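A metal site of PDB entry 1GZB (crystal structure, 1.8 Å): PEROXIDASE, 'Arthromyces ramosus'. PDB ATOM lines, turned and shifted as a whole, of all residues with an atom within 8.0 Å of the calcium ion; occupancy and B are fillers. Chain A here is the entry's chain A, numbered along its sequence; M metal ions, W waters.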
ATOM      1  N   ILE A  53      -7.060   2.596  -3.713  1.00  0.00           N
ATOM      2  CA  ILE A  53      -7.300   1.171  -3.490  1.00  0.00           C
ATOM      3  C   ILE A  53      -8.672   0.701  -3.959  1.00  0.00           C
ATOM      4  O   ILE A  53      -8.728  -0.286  -4.696  1.00  0.00           O
ATOM      5  CB  ILE A  53      -7.071   0.841  -1.992  1.00  0.00           C
ATOM      6  CG1 ILE A  53      -5.550   0.829  -1.716  1.00  0.00           C
ATOM      7  CG2 ILE A  53      -7.642  -0.531  -1.628  1.00  0.00           C
ATOM      8  CD1 ILE A  53      -5.157   0.871  -0.213  1.00  0.00           C
ATOM      9  N   VAL A  54      -9.780   1.345  -3.633  1.00  0.00           N
ATOM     10  CA  VAL A  54     -11.090   0.870  -4.048  1.00  0.00           C
ATOM     11  C   VAL A  54     -11.202   0.846  -5.582  1.00  0.00           C
ATOM     12  O   VAL A  54     -11.717  -0.111  -6.172  1.00  0.00           O
ATOM     13  CB  VAL A  54     -12.120   1.795  -3.342  1.00  0.00           C
ATOM     14  CG1 VAL A  54     -12.208   3.162  -4.011  1.00  0.00           C
ATOM     15  CG2 VAL A  54     -13.493   1.110  -3.388  1.00  0.00           C
ATOM     16  N   PHE A  55     -10.587   1.849  -6.250  1.00  0.00           N
ATOM     17  CA  PHE A  55     -10.591   1.939  -7.681  1.00  0.00           C
ATOM     18  C   PHE A  55      -9.764   0.771  -8.214  1.00  0.00           C
ATOM     19  O   PHE A  55     -10.284   0.001  -9.000  1.00  0.00           O
ATOM     20  CB  PHE A  55      -9.968   3.288  -8.152  1.00  0.00           C
ATOM     21  CG  PHE A  55      -9.826   3.491  -9.680  1.00  0.00           C
ATOM     22  CD1 PHE A  55     -10.793   3.059 -10.565  1.00  0.00           C
ATOM     23  CD2 PHE A  55      -8.662   4.038 -10.204  1.00  0.00           C
ATOM     24  CE1 PHE A  55     -10.594   3.173 -11.922  1.00  0.00           C
ATOM     25  CE2 PHE A  55      -8.464   4.144 -11.557  1.00  0.00           C
ATOM     26  CZ  PHE A  55      -9.427   3.709 -12.419  1.00  0.00           C
ATOM     27  N   HIS A  56      -8.513   0.576  -7.764  1.00  0.00           N
ATOM     28  CA  HIS A  56      -7.652  -0.479  -8.321  1.00  0.00           C
ATOM     29  C   HIS A  56      -8.133  -1.886  -8.014  1.00  0.00           C
ATOM     30  O   HIS A  56      -7.878  -2.817  -8.776  1.00  0.00           O
ATOM     31  CB  HIS A  56      -6.188  -0.300  -7.830  1.00  0.00           C
ATOM     32  CG  HIS A  56      -5.498   0.998  -8.275  1.00  0.00           C
ATOM     33  ND1 HIS A  56      -4.222   1.415  -7.859  1.00  0.00           N
ATOM     34  CD2 HIS A  56      -6.079   1.971  -9.098  1.00  0.00           C
ATOM     35  CE1 HIS A  56      -4.096   2.635  -8.407  1.00  0.00           C
ATOM     36  NE2 HIS A  56      -5.128   2.995  -9.106  1.00  0.00           N
ATOM     37  N   ASP A  57      -8.897  -2.036  -6.953  1.00  0.00           N
ATOM     38  CA  ASP A  57      -9.518  -3.321  -6.652  1.00  0.00           C
ATOM     39  C   ASP A  57     -10.709  -3.567  -7.597  1.00  0.00           C
ATOM     40  O   ASP A  57     -10.714  -4.600  -8.279  1.00  0.00           O
ATOM     41  CB  ASP A  57     -10.042  -3.398  -5.185  1.00  0.00           C
ATOM     42  CG  ASP A  57     -10.713  -4.731  -4.841  1.00  0.00           C
ATOM     43  OD1 ASP A  57     -10.303  -5.731  -5.405  1.00  0.00           O
ATOM     44  OD2 ASP A  57     -11.654  -4.775  -4.061  1.00  0.00           O
ATOM     45  N   ALA A  58     -11.667  -2.637  -7.727  1.00  0.00           N
ATOM     46  CA  ALA A  58     -12.865  -2.843  -8.528  1.00  0.00           C
ATOM     47  C   ALA A  58     -12.635  -2.885 -10.005  1.00  0.00           C
ATOM     48  O   ALA A  58     -13.324  -3.665 -10.676  1.00  0.00           O
ATOM     49  CB  ALA A  58     -13.888  -1.751  -8.301  1.00  0.00           C
ATOM     50  N   ILE A  59     -11.699  -2.059 -10.528  1.00  0.00           N
ATOM     51  CA  ILE A  59     -11.454  -2.020 -11.962  1.00  0.00           C
ATOM     52  C   ILE A  59     -10.773  -3.269 -12.534  1.00  0.00           C
ATOM     53  O   ILE A  59     -10.704  -3.407 -13.747  1.00  0.00           O
ATOM     54  CB  ILE A  59     -10.646  -0.687 -12.303  1.00  0.00           C
ATOM     55  CG1 ILE A  59     -11.082  -0.218 -13.698  1.00  0.00           C
ATOM     56  CG2 ILE A  59      -9.109  -0.888 -12.288  1.00  0.00           C
ATOM     57  CD1 ILE A  59     -12.560   0.265 -13.746  1.00  0.00           C
ATOM     58  N   GLY A  60     -10.298  -4.241 -11.747  1.00  0.00           N
ATOM     59  CA  GLY A  60      -9.706  -5.455 -12.291  1.00  0.00           C
ATOM     60  C   GLY A  60     -10.878  -6.332 -12.656  1.00  0.00           C
ATOM     61  O   GLY A  60     -11.212  -7.313 -11.976  1.00  0.00           O
ATOM     62  N   PHE A  61     -11.491  -5.996 -13.778  1.00  0.00           N
ATOM     63  CA  PHE A  61     -12.686  -6.703 -14.202  1.00  0.00           C
ATOM     64  C   PHE A  61     -12.786  -6.478 -15.715  1.00  0.00           C
ATOM     65  O   PHE A  61     -12.943  -5.324 -16.136  1.00  0.00           O
ATOM     66  CB  PHE A  61     -13.900  -6.089 -13.418  1.00  0.00           C
ATOM     67  CG  PHE A  61     -15.261  -6.679 -13.793  1.00  0.00           C
ATOM     68  CD1 PHE A  61     -15.558  -7.966 -13.433  1.00  0.00           C
ATOM     69  CD2 PHE A  61     -16.135  -5.924 -14.541  1.00  0.00           C
ATOM     70  CE1 PHE A  61     -16.757  -8.524 -13.849  1.00  0.00           C
ATOM     71  CE2 PHE A  61     -17.333  -6.477 -14.943  1.00  0.00           C
ATOM     72  CZ  PHE A  61     -17.641  -7.779 -14.600  1.00  0.00           C
ATOM     73  N   GLY A  73     -11.146 -11.226 -14.064  1.00  0.00           N
ATOM     74  CA  GLY A  73     -11.045 -10.427 -12.840  1.00  0.00           C
ATOM     75  C   GLY A  73     -12.354 -10.494 -12.070  1.00  0.00           C
ATOM     76  O   GLY A  73     -13.428 -10.676 -12.656  1.00  0.00           O
ATOM     77  N   GLY A  74     -12.317 -10.439 -10.751  1.00  0.00           N
ATOM     78  CA  GLY A  74     -13.534 -10.503  -9.946  1.00  0.00           C
ATOM     79  C   GLY A  74     -14.133  -9.142  -9.590  1.00  0.00           C
ATOM     80  O   GLY A  74     -15.199  -9.071  -8.959  1.00  0.00           O
ATOM     81  N   GLY A  75     -13.484  -8.043  -9.977  1.00  0.00           N
ATOM     82  CA  GLY A  75     -14.035  -6.744  -9.689  1.00  0.00           C
ATOM     83  C   GLY A  75     -13.790  -6.378  -8.243  1.00  0.00           C
ATOM     84  O   GLY A  75     -12.689  -6.611  -7.734  1.00  0.00           O
ATOM     85  N   ALA A  76     -14.813  -5.903  -7.547  1.00  0.00           N
ATOM     86  CA  ALA A  76     -14.728  -5.400  -6.188  1.00  0.00           C
ATOM     87  C   ALA A  76     -14.765  -6.564  -5.208  1.00  0.00           C
ATOM     88  O   ALA A  76     -15.609  -6.627  -4.309  1.00  0.00           O
ATOM     89  CB  ALA A  76     -15.916  -4.452  -5.929  1.00  0.00           C
ATOM     90  N   ASP A  77     -13.764  -7.442  -5.360  1.00  0.00           N
ATOM     91  CA  ASP A  77     -13.693  -8.661  -4.582  1.00  0.00           C
ATOM     92  C   ASP A  77     -12.597  -8.669  -3.501  1.00  0.00           C
ATOM     93  O   ASP A  77     -12.309  -9.704  -2.873  1.00  0.00           O
ATOM     94  CB  ASP A  77     -13.499  -9.796  -5.580  1.00  0.00           C
ATOM     95  CG  ASP A  77     -12.222  -9.728  -6.419  1.00  0.00           C
ATOM     96  OD1 ASP A  77     -11.481  -8.748  -6.365  1.00  0.00           O
ATOM     97  OD2 ASP A  77     -11.943 -10.673  -7.146  1.00  0.00           O
ATOM     98  N   GLY A  78     -11.913  -7.526  -3.327  1.00  0.00           N
ATOM     99  CA  GLY A  78     -10.823  -7.428  -2.342  1.00  0.00           C
ATOM    100  C   GLY A  78      -9.587  -8.250  -2.699  1.00  0.00           C
ATOM    101  O   GLY A  78      -8.725  -8.450  -1.823  1.00  0.00           O
ATOM    102  N   SER A  79      -9.420  -8.616  -3.976  1.00  0.00           N
ATOM    103  CA  SER A  79      -8.285  -9.405  -4.450  1.00  0.00           C
ATOM    104  C   SER A  79      -6.979  -8.645  -4.233  1.00  0.00           C
ATOM    105  O   SER A  79      -5.937  -9.281  -4.148  1.00  0.00           O
ATOM    106  CB  SER A  79      -8.404  -9.733  -5.915  1.00  0.00           C
ATOM    107  OG  SER A  79      -8.480  -8.543  -6.712  1.00  0.00           O
ATOM    108  N   ILE A  80      -7.004  -7.273  -4.205  1.00  0.00           N
ATOM    109  CA  ILE A  80      -5.782  -6.524  -3.959  1.00  0.00           C
ATOM    110  C   ILE A  80      -5.226  -6.751  -2.551  1.00  0.00           C
ATOM    111  O   ILE A  80      -4.031  -6.545  -2.322  1.00  0.00           O
ATOM    112  CB  ILE A  80      -6.121  -5.021  -4.263  1.00  0.00           C
ATOM    113  CG1 ILE A  80      -4.841  -4.177  -4.262  1.00  0.00           C
ATOM    114  CG2 ILE A  80      -7.156  -4.522  -3.271  1.00  0.00           C
ATOM    115  CD1 ILE A  80      -4.992  -2.863  -5.046  1.00  0.00           C
ATOM    116  N   ILE A  81      -6.048  -7.213  -1.584  1.00  0.00           N
ATOM    117  CA  ILE A  81      -5.539  -7.508  -0.261  1.00  0.00           C
ATOM    118  C   ILE A  81      -5.150  -8.995  -0.240  1.00  0.00           C
ATOM    119  O   ILE A  81      -4.011  -9.377   0.037  1.00  0.00           O
ATOM    120  CB  ILE A  81      -6.598  -7.191   0.812  1.00  0.00           C
ATOM    121  CG1 ILE A  81      -7.003  -5.721   0.767  1.00  0.00           C
ATOM    122  CG2 ILE A  81      -6.014  -7.567   2.172  1.00  0.00           C
ATOM    123  CD1 ILE A  81      -7.762  -5.221   2.009  1.00  0.00           C
ATOM    124  N   HIS A  83      -4.523 -11.156  -2.555  1.00  0.00           N
ATOM    125  CA  HIS A  83      -3.467 -11.484  -3.495  1.00  0.00           C
ATOM    126  C   HIS A  83      -2.571 -10.269  -3.692  1.00  0.00           C
ATOM    127  O   HIS A  83      -2.162  -9.935  -4.793  1.00  0.00           O
ATOM    128  CB  HIS A  83      -4.103 -11.933  -4.788  1.00  0.00           C
ATOM    129  CG  HIS A  83      -5.004 -13.128  -4.545  1.00  0.00           C
ATOM    130  ND1 HIS A  83      -4.609 -14.468  -4.324  1.00  0.00           N
ATOM    131  CD2 HIS A  83      -6.397 -13.043  -4.618  1.00  0.00           C
ATOM    132  CE1 HIS A  83      -5.790 -15.164  -4.333  1.00  0.00           C
ATOM    133  NE2 HIS A  83      -6.798 -14.366  -4.492  1.00  0.00           N
ATOM    134  N   GLU A  87      -0.737  -8.475  -6.989  1.00  0.00           N
ATOM    135  CA  GLU A  87      -1.248  -7.186  -7.430  1.00  0.00           C
ATOM    136  C   GLU A  87      -0.428  -5.950  -7.108  1.00  0.00           C
ATOM    137  O   GLU A  87      -0.435  -4.957  -7.858  1.00  0.00           O
ATOM    138  CB  GLU A  87      -2.620  -6.910  -6.864  1.00  0.00           C
ATOM    139  CG  GLU A  87      -3.563  -7.829  -7.570  1.00  0.00           C
ATOM    140  CD  GLU A  87      -5.028  -7.470  -7.453  1.00  0.00           C
ATOM    141  OE1 GLU A  87      -5.366  -6.274  -7.367  1.00  0.00           O
ATOM    142  OE2 GLU A  87      -5.818  -8.424  -7.448  1.00  0.00           O
ATOM    143  N   GLY A 115     -13.423  -7.547   0.299  1.00  0.00           N
ATOM    144  CA  GLY A 115     -14.153  -6.728  -0.693  1.00  0.00           C
ATOM    145  C   GLY A 115     -15.141  -5.768  -0.064  1.00  0.00           C
ATOM    146  O   GLY A 115     -15.241  -4.612  -0.472  1.00  0.00           O
ATOM    147  N   ILE A 118     -13.121  -2.910   1.885  1.00  0.00           N
ATOM    148  CA  ILE A 118     -12.595  -1.820   1.079  1.00  0.00           C
ATOM    149  C   ILE A 118     -13.696  -0.828   0.769  1.00  0.00           C
ATOM    150  O   ILE A 118     -13.479   0.369   0.951  1.00  0.00           O
ATOM    151  CB  ILE A 118     -11.986  -2.375  -0.174  1.00  0.00           C
ATOM    152  CG1 ILE A 118     -10.649  -3.022   0.173  1.00  0.00           C
ATOM    153  CG2 ILE A 118     -11.703  -1.245  -1.141  1.00  0.00           C
ATOM    154  CD1 ILE A 118      -9.962  -3.780  -0.985  1.00  0.00           C
ATOM    155  N   SER A 145     -11.352 -14.786  -3.749  1.00  0.00           N
ATOM    156  CA  SER A 145     -11.010 -14.068  -4.956  1.00  0.00           C
ATOM    157  C   SER A 145      -9.855 -14.765  -5.651  1.00  0.00           C
ATOM    158  O   SER A 145      -9.170 -15.640  -5.123  1.00  0.00           O
ATOM    159  CB  SER A 145     -10.625 -12.629  -4.594  1.00  0.00           C
ATOM    160  OG  SER A 145      -9.580 -12.609  -3.637  1.00  0.00           O
ATOM    161  N   GLN A 146      -9.769 -14.490  -6.931  1.00  0.00           N
ATOM    162  CA  GLN A 146      -8.655 -14.945  -7.737  1.00  0.00           C
ATOM    163  C   GLN A 146      -7.815 -13.679  -7.900  1.00  0.00           C
ATOM    164  O   GLN A 146      -8.371 -12.563  -7.736  1.00  0.00           O
ATOM    165  CB  GLN A 146      -9.146 -15.405  -9.077  1.00  0.00           C
ATOM    166  CG  GLN A 146      -9.206 -16.923  -9.082  1.00  0.00           C
ATOM    167  CD  GLN A 146     -10.233 -17.401 -10.115  1.00  0.00           C
ATOM    168  OE1 GLN A 146      -9.946 -17.597 -11.311  1.00  0.00           O
ATOM    169  NE2 GLN A 146     -11.473 -17.583  -9.612  1.00  0.00           N
ATOM    170  N   PRO A 147      -6.515 -13.711  -8.158  1.00  0.00           N
ATOM    171  CA  PRO A 147      -5.752 -12.496  -8.435  1.00  0.00           C
ATOM    172  C   PRO A 147      -6.260 -11.840  -9.742  1.00  0.00           C
ATOM    173  O   PRO A 147      -6.649 -12.521 -10.691  1.00  0.00           O
ATOM    174  CB  PRO A 147      -4.330 -12.969  -8.504  1.00  0.00           C
ATOM    175  CG  PRO A 147      -4.431 -14.424  -8.922  1.00  0.00           C
ATOM    176  CD  PRO A 147      -5.681 -14.915  -8.204  1.00  0.00           C
ATOM    177  N   SER A 148      -6.330 -10.515  -9.747  1.00  0.00           N
ATOM    178  CA  SER A 148      -6.746  -9.729 -10.896  1.00  0.00           C
ATOM    179  C   SER A 148      -5.732  -9.999 -12.018  1.00  0.00           C
ATOM    180  O   SER A 148      -4.523 -10.204 -11.753  1.00  0.00           O
ATOM    181  CB  SER A 148      -6.738  -8.229 -10.562  1.00  0.00           C
ATOM    182  OG  SER A 148      -6.823  -7.313 -11.653  1.00  0.00           O
ATOM    183  N   PRO A 149      -6.195 -10.029 -13.264  1.00  0.00           N
ATOM    184  CA  PRO A 149      -5.327 -10.080 -14.400  1.00  0.00           C
ATOM    185  C   PRO A 149      -4.482  -8.782 -14.401  1.00  0.00           C
ATOM    186  O   PRO A 149      -4.916  -7.762 -13.829  1.00  0.00           O
ATOM    187  CB  PRO A 149      -6.292 -10.216 -15.565  1.00  0.00           C
ATOM    188  CG  PRO A 149      -7.425 -11.026 -14.958  1.00  0.00           C
ATOM    189  CD  PRO A 149      -7.567 -10.256 -13.655  1.00  0.00           C
ATOM    190  N   LEU A 283     -19.040  -4.039  -9.258  1.00  0.00           N
ATOM    191  CA  LEU A 283     -18.414  -4.711 -10.380  1.00  0.00           C
ATOM    192  C   LEU A 283     -18.062  -6.156  -9.955  1.00  0.00           C
ATOM    193  O   LEU A 283     -17.434  -6.419  -8.916  1.00  0.00           O
ATOM    194  CB  LEU A 283     -17.155  -3.930 -10.766  1.00  0.00           C
ATOM    195  CG  LEU A 283     -17.136  -2.981 -12.010  1.00  0.00           C
ATOM    196  CD1 LEU A 283     -18.406  -2.230 -12.225  1.00  0.00           C
ATOM    197  CD2 LEU A 283     -15.946  -2.036 -11.819  1.00  0.00           C
ATOM    198  N   PHE A 285     -20.449  -8.325  -9.181  1.00  0.00           N
ATOM    199  CA  PHE A 285     -21.469  -8.767  -8.230  1.00  0.00           C
ATOM    200  C   PHE A 285     -22.852  -8.382  -8.676  1.00  0.00           C
ATOM    201  O   PHE A 285     -22.995  -7.546  -9.565  1.00  0.00           O
ATOM    202  CB  PHE A 285     -21.260  -8.150  -6.816  1.00  0.00           C
ATOM    203  CG  PHE A 285     -20.019  -8.765  -6.204  1.00  0.00           C
ATOM    204  CD1 PHE A 285     -18.767  -8.207  -6.461  1.00  0.00           C
ATOM    205  CD2 PHE A 285     -20.128  -9.958  -5.476  1.00  0.00           C
ATOM    206  CE1 PHE A 285     -17.627  -8.858  -6.000  1.00  0.00           C
ATOM    207  CE2 PHE A 285     -18.984 -10.591  -5.022  1.00  0.00           C
ATOM    208  CZ  PHE A 285     -17.748 -10.045  -5.290  1.00  0.00           C
HETATM  209 CA    CA M   1     -10.236  -6.896  -7.447  1.00  0.00          CA
HETATM  210  O   HOH W   1      -8.079  -5.692  -8.253  1.00  0.00           O
HETATM  211  O   HOH W   2      -9.959  -8.061  -9.603  1.00  0.00           O
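Of the 29 residues printed, 4 come within 4 Å of the calcium ion.
Along chain A the residues within 4 Å of the calcium ion span positions 57 to 79.
The backbone NH (N) of Gly 78 lies within hydrogen-bond range of the side-chain carboxylate (OD2) of Asp 57 (2.9 Å).
The backbone carbonyl oxygen (O) of Gly 60 lies within hydrogen-bond range of the backbone NH (N) of Gly 75, at 3.1 Å.
The side-chain carboxylate (OE2) of Glu 87 lies close to the side-chain hydroxyl (OG) of Ser 79 (2.8 Å).
The calcium ion is bound by OD1 of Asp 57 (2.4 Å), water W2 (2.5 Å), OD1 of Asp 77 (2.5 Å), O of Gly 75 (2.5 Å), O of Asp 57 (2.5 Å), OG of Ser 79 (2.5 Å) and water W1 (2.6 Å).
Water W1 bridges OE1 of Glu 87 and O of His 56.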
